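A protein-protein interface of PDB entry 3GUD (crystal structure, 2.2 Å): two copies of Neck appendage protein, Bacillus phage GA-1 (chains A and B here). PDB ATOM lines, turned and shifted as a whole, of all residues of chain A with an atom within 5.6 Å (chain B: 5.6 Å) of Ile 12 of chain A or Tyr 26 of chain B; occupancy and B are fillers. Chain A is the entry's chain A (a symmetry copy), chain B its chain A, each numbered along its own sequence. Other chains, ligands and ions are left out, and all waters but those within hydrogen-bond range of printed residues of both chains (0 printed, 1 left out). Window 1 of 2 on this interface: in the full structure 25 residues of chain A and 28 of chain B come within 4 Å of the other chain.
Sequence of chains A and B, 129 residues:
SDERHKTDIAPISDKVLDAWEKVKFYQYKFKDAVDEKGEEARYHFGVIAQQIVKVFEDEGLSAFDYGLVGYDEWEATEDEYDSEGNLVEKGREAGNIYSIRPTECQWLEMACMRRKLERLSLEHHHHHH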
ATOM      1  N   ILE A   9      30.991   8.260  -2.196  1.00  0.00           N
ATOM      2  CA  ILE A   9      31.100   8.383  -3.633  1.00  0.00           C
ATOM      3  C   ILE A   9      30.211   7.341  -4.305  1.00  0.00           C
ATOM      4  O   ILE A   9      30.192   6.167  -3.916  1.00  0.00           O
ATOM      5  CB  ILE A   9      32.561   8.211  -4.055  1.00  0.00           C
ATOM      6  CG1 ILE A   9      32.833   8.941  -5.365  1.00  0.00           C
ATOM      7  CG2 ILE A   9      32.898   6.745  -4.143  1.00  0.00           C
ATOM      8  CD1 ILE A   9      32.050   8.382  -6.536  1.00  0.00           C
ATOM      9  N   ALA A  10      29.448   7.781  -5.299  1.00  0.00           N
ATOM     10  CA  ALA A  10      28.498   6.895  -5.944  1.00  0.00           C
ATOM     11  C   ALA A  10      27.797   7.587  -7.087  1.00  0.00           C
ATOM     12  O   ALA A  10      27.891   8.802  -7.241  1.00  0.00           O
ATOM     13  CB  ALA A  10      27.479   6.406  -4.938  1.00  0.00           C
ATOM     14  N   PRO A  11      27.093   6.810  -7.907  1.00  0.00           N
ATOM     15  CA  PRO A  11      26.306   7.415  -8.977  1.00  0.00           C
ATOM     16  C   PRO A  11      25.207   8.281  -8.376  1.00  0.00           C
ATOM     17  O   PRO A  11      24.947   8.213  -7.176  1.00  0.00           O
ATOM     18  CB  PRO A  11      25.731   6.203  -9.707  1.00  0.00           C
ATOM     19  CG  PRO A  11      26.694   5.082  -9.390  1.00  0.00           C
ATOM     20  CD  PRO A  11      27.104   5.341  -7.979  1.00  0.00           C
ATOM     21  N   ILE A  12      24.570   9.094  -9.204  1.00  0.00           N
ATOM     22  CA  ILE A  12      23.669  10.121  -8.701  1.00  0.00           C
ATOM     23  C   ILE A  12      22.279   9.593  -8.308  1.00  0.00           C
ATOM     24  O   ILE A  12      21.580   8.961  -9.107  1.00  0.00           O
ATOM     25  CB  ILE A  12      23.564  11.301  -9.704  1.00  0.00           C
ATOM     26  CG1 ILE A  12      24.947  11.938  -9.903  1.00  0.00           C
ATOM     27  CG2 ILE A  12      22.517  12.335  -9.243  1.00  0.00           C
ATOM     28  CD1 ILE A  12      25.050  12.813 -11.119  1.00  0.00           C
ATOM     29  N   SER A  13      21.910   9.861  -7.055  1.00  0.00           N
ATOM     30  CA  SER A  13      20.585   9.570  -6.511  1.00  0.00           C
ATOM     31  C   SER A  13      19.488   9.796  -7.549  1.00  0.00           C
ATOM     32  O   SER A  13      19.560  10.732  -8.359  1.00  0.00           O
ATOM     33  CB  SER A  13      20.337  10.439  -5.269  1.00  0.00           C
ATOM     34  OG  SER A  13      19.088  10.163  -4.671  1.00  0.00           O
ATOM     35  N   ASP A  14      18.484   8.922  -7.525  1.00  0.00           N
ATOM     36  CA  ASP A  14      17.407   8.934  -8.518  1.00  0.00           C
ATOM     37  C   ASP A  14      16.253   9.806  -8.055  1.00  0.00           C
ATOM     38  O   ASP A  14      15.595  10.455  -8.858  1.00  0.00           O
ATOM     39  CB  ASP A  14      16.899   7.513  -8.767  1.00  0.00           C
ATOM     40  CG  ASP A  14      17.513   6.869  -9.988  1.00  0.00           C
ATOM     41  OD1 ASP A  14      17.498   7.497 -11.076  1.00  0.00           O
ATOM     42  OD2 ASP A  14      17.979   5.717  -9.848  1.00  0.00           O
ATOM     43  N   VAL A  16      16.816  12.404  -6.261  1.00  0.00           N
ATOM     44  CA  VAL A  16      17.416  13.703  -6.590  1.00  0.00           C
ATOM     45  C   VAL A  16      17.210  14.079  -8.058  1.00  0.00           C
ATOM     46  O   VAL A  16      16.693  15.151  -8.369  1.00  0.00           O
ATOM     47  CB  VAL A  16      18.920  13.716  -6.287  1.00  0.00           C
ATOM     48  CG1 VAL A  16      19.542  15.054  -6.682  1.00  0.00           C
ATOM     49  CG2 VAL A  16      19.146  13.433  -4.818  1.00  0.00           C
ATOM     50  N   LEU A  17      17.621  13.192  -8.955  1.00  0.00           N
ATOM     51  CA  LEU A  17      17.496  13.432 -10.383  1.00  0.00           C
ATOM     52  C   LEU A  17      16.028  13.612 -10.723  1.00  0.00           C
ATOM     53  O   LEU A  17      15.662  14.343 -11.641  1.00  0.00           O
ATOM     54  CB  LEU A  17      18.089  12.249 -11.142  1.00  0.00           C
ATOM     55  CG  LEU A  17      18.878  12.516 -12.427  1.00  0.00           C
ATOM     56  CD1 LEU A  17      19.601  13.844 -12.360  1.00  0.00           C
ATOM     57  CD2 LEU A  17      19.861  11.389 -12.703  1.00  0.00           C
ATOM     58  N   LEU A 108      23.828  18.650 -12.356  1.00  0.00           N
ATOM     59  CA  LEU A 108      22.639  17.822 -12.174  1.00  0.00           C
ATOM     60  C   LEU A 108      21.735  17.874 -13.393  1.00  0.00           C
ATOM     61  O   LEU A 108      21.120  16.875 -13.761  1.00  0.00           O
ATOM     62  CB  LEU A 108      21.862  18.226 -10.914  1.00  0.00           C
ATOM     63  CG  LEU A 108      20.504  17.557 -10.682  1.00  0.00           C
ATOM     64  CD1 LEU A 108      20.666  16.053 -10.651  1.00  0.00           C
ATOM     65  CD2 LEU A 108      19.862  18.055  -9.393  1.00  0.00           C
ATOM     66  N   ALA A 111      23.384  15.555 -15.894  1.00  0.00           N
ATOM     67  CA  ALA A 111      23.207  14.170 -15.447  1.00  0.00           C
ATOM     68  C   ALA A 111      21.776  13.710 -15.709  1.00  0.00           C
ATOM     69  O   ALA A 111      21.532  12.543 -16.030  1.00  0.00           O
ATOM     70  CB  ALA A 111      23.545  14.033 -13.968  1.00  0.00           C
ATOM     71  N   LYS B  24      32.019   9.115 -16.424  1.00  0.00           N
ATOM     72  CA  LYS B  24      30.812   8.942 -15.599  1.00  0.00           C
ATOM     73  C   LYS B  24      30.515  10.163 -14.724  1.00  0.00           C
ATOM     74  O   LYS B  24      31.422  10.894 -14.345  1.00  0.00           O
ATOM     75  CB  LYS B  24      30.938   7.704 -14.692  1.00  0.00           C
ATOM     76  CG  LYS B  24      31.294   6.376 -15.380  1.00  0.00           C
ATOM     77  CD  LYS B  24      31.257   5.216 -14.374  1.00  0.00           C
ATOM     78  CE  LYS B  24      32.069   3.984 -14.821  1.00  0.00           C
ATOM     79  NZ  LYS B  24      33.480   3.943 -14.305  1.00  0.00           N
ATOM     80  N   PHE B  25      29.244  10.383 -14.402  1.00  0.00           N
ATOM     81  CA  PHE B  25      28.876  11.378 -13.397  1.00  0.00           C
ATOM     82  C   PHE B  25      28.668  10.709 -12.024  1.00  0.00           C
ATOM     83  O   PHE B  25      28.079   9.623 -11.940  1.00  0.00           O
ATOM     84  CB  PHE B  25      27.591  12.115 -13.791  1.00  0.00           C
ATOM     85  CG  PHE B  25      27.712  12.961 -15.026  1.00  0.00           C
ATOM     86  CD1 PHE B  25      28.940  13.443 -15.441  1.00  0.00           C
ATOM     87  CD2 PHE B  25      26.575  13.303 -15.753  1.00  0.00           C
ATOM     88  CE1 PHE B  25      29.039  14.233 -16.576  1.00  0.00           C
ATOM     89  CE2 PHE B  25      26.663  14.091 -16.884  1.00  0.00           C
ATOM     90  CZ  PHE B  25      27.895  14.553 -17.300  1.00  0.00           C
ATOM     91  N   TYR B  26      29.135  11.373 -10.958  1.00  0.00           N
ATOM     92  CA  TYR B  26      29.008  10.889  -9.575  1.00  0.00           C
ATOM     93  C   TYR B  26      28.376  11.901  -8.624  1.00  0.00           C
ATOM     94  O   TYR B  26      28.377  13.104  -8.883  1.00  0.00           O
ATOM     95  CB  TYR B  26      30.383  10.567  -8.998  1.00  0.00           C
ATOM     96  CG  TYR B  26      31.126   9.463  -9.696  1.00  0.00           C
ATOM     97  CD1 TYR B  26      31.057   8.156  -9.239  1.00  0.00           C
ATOM     98  CD2 TYR B  26      31.911   9.733 -10.806  1.00  0.00           C
ATOM     99  CE1 TYR B  26      31.737   7.159  -9.873  1.00  0.00           C
ATOM    100  CE2 TYR B  26      32.594   8.740 -11.444  1.00  0.00           C
ATOM    101  CZ  TYR B  26      32.505   7.460 -10.977  1.00  0.00           C
ATOM    102  OH  TYR B  26      33.199   6.480 -11.627  1.00  0.00           O
ATOM    103  N   GLN B  27      27.846  11.399  -7.513  1.00  0.00           N
ATOM    104  CA  GLN B  27      27.597  12.234  -6.349  1.00  0.00           C
ATOM    105  C   GLN B  27      28.521  11.720  -5.263  1.00  0.00           C
ATOM    106  O   GLN B  27      28.790  10.526  -5.180  1.00  0.00           O
ATOM    107  CB  GLN B  27      26.124  12.227  -5.922  1.00  0.00           C
ATOM    108  CG  GLN B  27      25.721  11.157  -4.917  1.00  0.00           C
ATOM    109  CD  GLN B  27      24.227  11.208  -4.584  1.00  0.00           C
ATOM    110  OE1 GLN B  27      23.394  11.479  -5.447  1.00  0.00           O
ATOM    111  NE2 GLN B  27      23.890  10.947  -3.327  1.00  0.00           N
ATOM    112  N   TYR B  28      29.047  12.641  -4.466  1.00  0.00           N
ATOM    113  CA  TYR B  28      30.055  12.326  -3.455  1.00  0.00           C
ATOM    114  C   TYR B  28      30.097  13.451  -2.418  1.00  0.00           C
ATOM    115  O   TYR B  28      29.521  14.520  -2.615  1.00  0.00           O
ATOM    116  CB  TYR B  28      31.437  12.168  -4.109  1.00  0.00           C
ATOM    117  CG  TYR B  28      31.763  13.301  -5.066  1.00  0.00           C
ATOM    118  CD1 TYR B  28      32.345  14.483  -4.611  1.00  0.00           C
ATOM    119  CD2 TYR B  28      31.455  13.204  -6.422  1.00  0.00           C
ATOM    120  CE1 TYR B  28      32.624  15.536  -5.494  1.00  0.00           C
ATOM    121  CE2 TYR B  28      31.731  14.245  -7.306  1.00  0.00           C
ATOM    122  CZ  TYR B  28      32.315  15.407  -6.840  1.00  0.00           C
ATOM    123  OH  TYR B  28      32.591  16.443  -7.719  1.00  0.00           O
ATOM    124  N   HIS B  44      27.621  16.891  -3.531  1.00  0.00           N
ATOM    125  CA  HIS B  44      28.001  17.596  -4.761  1.00  0.00           C
ATOM    126  C   HIS B  44      27.971  16.636  -5.939  1.00  0.00           C
ATOM    127  O   HIS B  44      28.240  15.450  -5.785  1.00  0.00           O
ATOM    128  CB  HIS B  44      29.392  18.223  -4.653  1.00  0.00           C
ATOM    129  CG  HIS B  44      29.501  19.258  -3.584  1.00  0.00           C
ATOM    130  ND1 HIS B  44      30.648  19.439  -2.830  1.00  0.00           N
ATOM    131  CD2 HIS B  44      28.609  20.161  -3.119  1.00  0.00           C
ATOM    132  CE1 HIS B  44      30.456  20.408  -1.963  1.00  0.00           C
ATOM    133  NE2 HIS B  44      29.222  20.869  -2.115  1.00  0.00           N
ATOM    134  N   PHE B  45      27.635  17.154  -7.114  1.00  0.00           N
ATOM    135  CA  PHE B  45      27.510  16.327  -8.306  1.00  0.00           C
ATOM    136  C   PHE B  45      28.580  16.726  -9.305  1.00  0.00           C
ATOM    137  O   PHE B  45      28.848  17.912  -9.480  1.00  0.00           O
ATOM    138  CB  PHE B  45      26.128  16.508  -8.948  1.00  0.00           C
ATOM    139  CG  PHE B  45      24.984  16.508  -7.962  1.00  0.00           C
ATOM    140  CD1 PHE B  45      24.034  17.515  -7.985  1.00  0.00           C
ATOM    141  CD2 PHE B  45      24.860  15.511  -7.014  1.00  0.00           C
ATOM    142  CE1 PHE B  45      22.983  17.522  -7.087  1.00  0.00           C
ATOM    143  CE2 PHE B  45      23.812  15.521  -6.115  1.00  0.00           C
ATOM    144  CZ  PHE B  45      22.875  16.529  -6.160  1.00  0.00           C
ATOM    145  N   GLY B  46      29.196  15.750  -9.961  1.00  0.00           N
ATOM    146  CA  GLY B  46      30.117  16.078 -11.028  1.00  0.00           C
ATOM    147  C   GLY B  46      30.876  14.916 -11.616  1.00  0.00           C
ATOM    148  O   GLY B  46      30.453  13.781 -11.540  1.00  0.00           O
ATOM    149  N   VAL B  47      32.014  15.218 -12.218  1.00  0.00           N
ATOM    150  CA  VAL B  47      32.875  14.200 -12.804  1.00  0.00           C
ATOM    151  C   VAL B  47      34.074  13.990 -11.886  1.00  0.00           C
ATOM    152  O   VAL B  47      34.269  14.754 -10.938  1.00  0.00           O
ATOM    153  CB  VAL B  47      33.336  14.594 -14.236  1.00  0.00           C
ATOM    154  CG1 VAL B  47      32.188  14.447 -15.222  1.00  0.00           C
ATOM    155  CG2 VAL B  47      33.870  16.011 -14.252  1.00  0.00           C
ATOM    156  N   ILE B  48      34.865  12.953 -12.153  1.00  0.00           N
ATOM    157  CA  ILE B  48      36.034  12.660 -11.327  1.00  0.00           C
ATOM    158  C   ILE B  48      37.309  12.546 -12.168  1.00  0.00           C
ATOM    159  O   ILE B  48      37.427  11.655 -13.002  1.00  0.00           O
ATOM    160  CB  ILE B  48      35.821  11.376 -10.498  1.00  0.00           C
ATOM    161  CG1 ILE B  48      34.745  11.603  -9.432  1.00  0.00           C
ATOM    162  CG2 ILE B  48      37.132  10.920  -9.858  1.00  0.00           C
ATOM    163  CD1 ILE B  48      34.444  10.377  -8.607  1.00  0.00           C
ATOM    164  N   GLN B  51      39.170   9.223 -13.131  1.00  0.00           N
ATOM    165  CA  GLN B  51      38.439   8.419 -14.075  1.00  0.00           C
ATOM    166  C   GLN B  51      38.497   9.006 -15.484  1.00  0.00           C
ATOM    167  O   GLN B  51      38.510   8.264 -16.470  1.00  0.00           O
ATOM    168  CB  GLN B  51      36.987   8.354 -13.709  1.00  0.00           C
ATOM    169  CG  GLN B  51      36.202   8.737 -14.915  1.00  0.00           C
ATOM    170  CD  GLN B  51      34.908   8.066 -14.964  1.00  0.00           C
ATOM    171  OE1 GLN B  51      34.470   7.482 -13.976  1.00  0.00           O
ATOM    172  NE2 GLN B  51      34.259   8.129 -16.112  1.00  0.00           N
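The backbone NH (N) of Ser 13 of chain A sits at hydrogen-bond distance from the side-chain amide oxygen (OE1) of Gln 27 of chain B (2.7 Å).
The backbone NH of Gln 27 of chain B is in hydrogen-bond range of the backbone carbonyl oxygen of Ala 10 of chain A (2.6 Å).
N of Tyr 26 of chain B lies within hydrogen-bond range of O of Gly 46 of chain B (2.8 Å).
The side-chain hydroxyl (OH) of Tyr 26 of chain B is in hydrogen-bond range of the side-chain amide oxygen (OE1) of Gln 51 of chain B (2.9 Å).
The backbone carbonyl oxygen of Tyr 28 of chain B is in hydrogen-bond range of the backbone NH of His 44 of chain B, 3.2 Å away.
Among the printed residues, pairs that only touch across the chains: Ile 9 of chain A with Tyr 26 of chain B (2.9 Å), Ile 9 of chain A with Gln 27 of chain B (3.5 Å), Ile 9 of chain A with Tyr 28 of chain B (3.7 Å), Ile 9 of chain A with Ile 48 of chain B (3.7 Å), Ala 10 of chain A with Tyr 26 of chain B (3.3 Å), Pro 11 of chain A with Gln 27 of chain B (3.8 Å), Ile 12 of chain A with Phe 25 of chain B (3.8 Å), Ile 12 of chain A with Tyr 26 of chain B (3.7 Å), Ile 12 of chain A with Gln 27 of chain B (3.5 Å), Val 16 of chain A with Phe 45 of chain B (3.7 Å), Leu 108 of chain A with Phe 45 of chain B (3.7 Å) and Ala 111 of chain A with Phe 25 of chain B (3.5 Å).
Printed residues of chain B within 4 Å of Ala 10 of chain A: Tyr 26 (3.3 Å) and Gln 27 (2.6 Å).
Of the printed residues of chain B, Pro 11 of chain A touches Gln 27.
Of the printed residues of chain B, Leu 108 of chain A touches Phe 45.
Of the printed residues of chain B, Ala 111 of chain A touches Phe 25.
Tyr 26 of chain B touches three residues of chain A.
Of the printed residues of chain A, Gln 27 of chain B touches Ile 9 (3.5 Å), Ala 10 (2.6 Å), Pro 11 (3.8 Å), Ile 12 (3.5 Å) and Ser 13 (2.7 Å).
The nearest residue of chain B that does not touch Ile 12 of chain A is Phe 45 of chain B (4.4 Å).
The nearest residue of chain A that does not touch Tyr 26 of chain B is Pro 11 of chain A (4.4 Å).
The nearest printed residue of chain A that does not touch Phe 25 of chain B is Pro 11 of chain A (4.1 Å).
Of the 10 printed residues of chain A, 8 touch a printed residue of chain B.
Printed residues of chain A that touch a printed residue of chain B: Ile 9, Ala 10, Pro 11, Ile 12, Ser 13, Val 16, Leu 108 and Ala 111.
Hydrophobic or aromatic side chains of chain A that line the printed part of chain B: Ile 9, Ile 12, Val 16, Leu 108 and Ala 111.
Hydrophobic or aromatic side chains of chain B within 4 Å of the printed part of chain A: Phe 25, Tyr 26, Tyr 28, Phe 45 and Ile 48.
No position is printed for both chains.
Of the 14 pairs that touch across the chains among the printed residues, none has its exchanged pair printed and touching as well.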
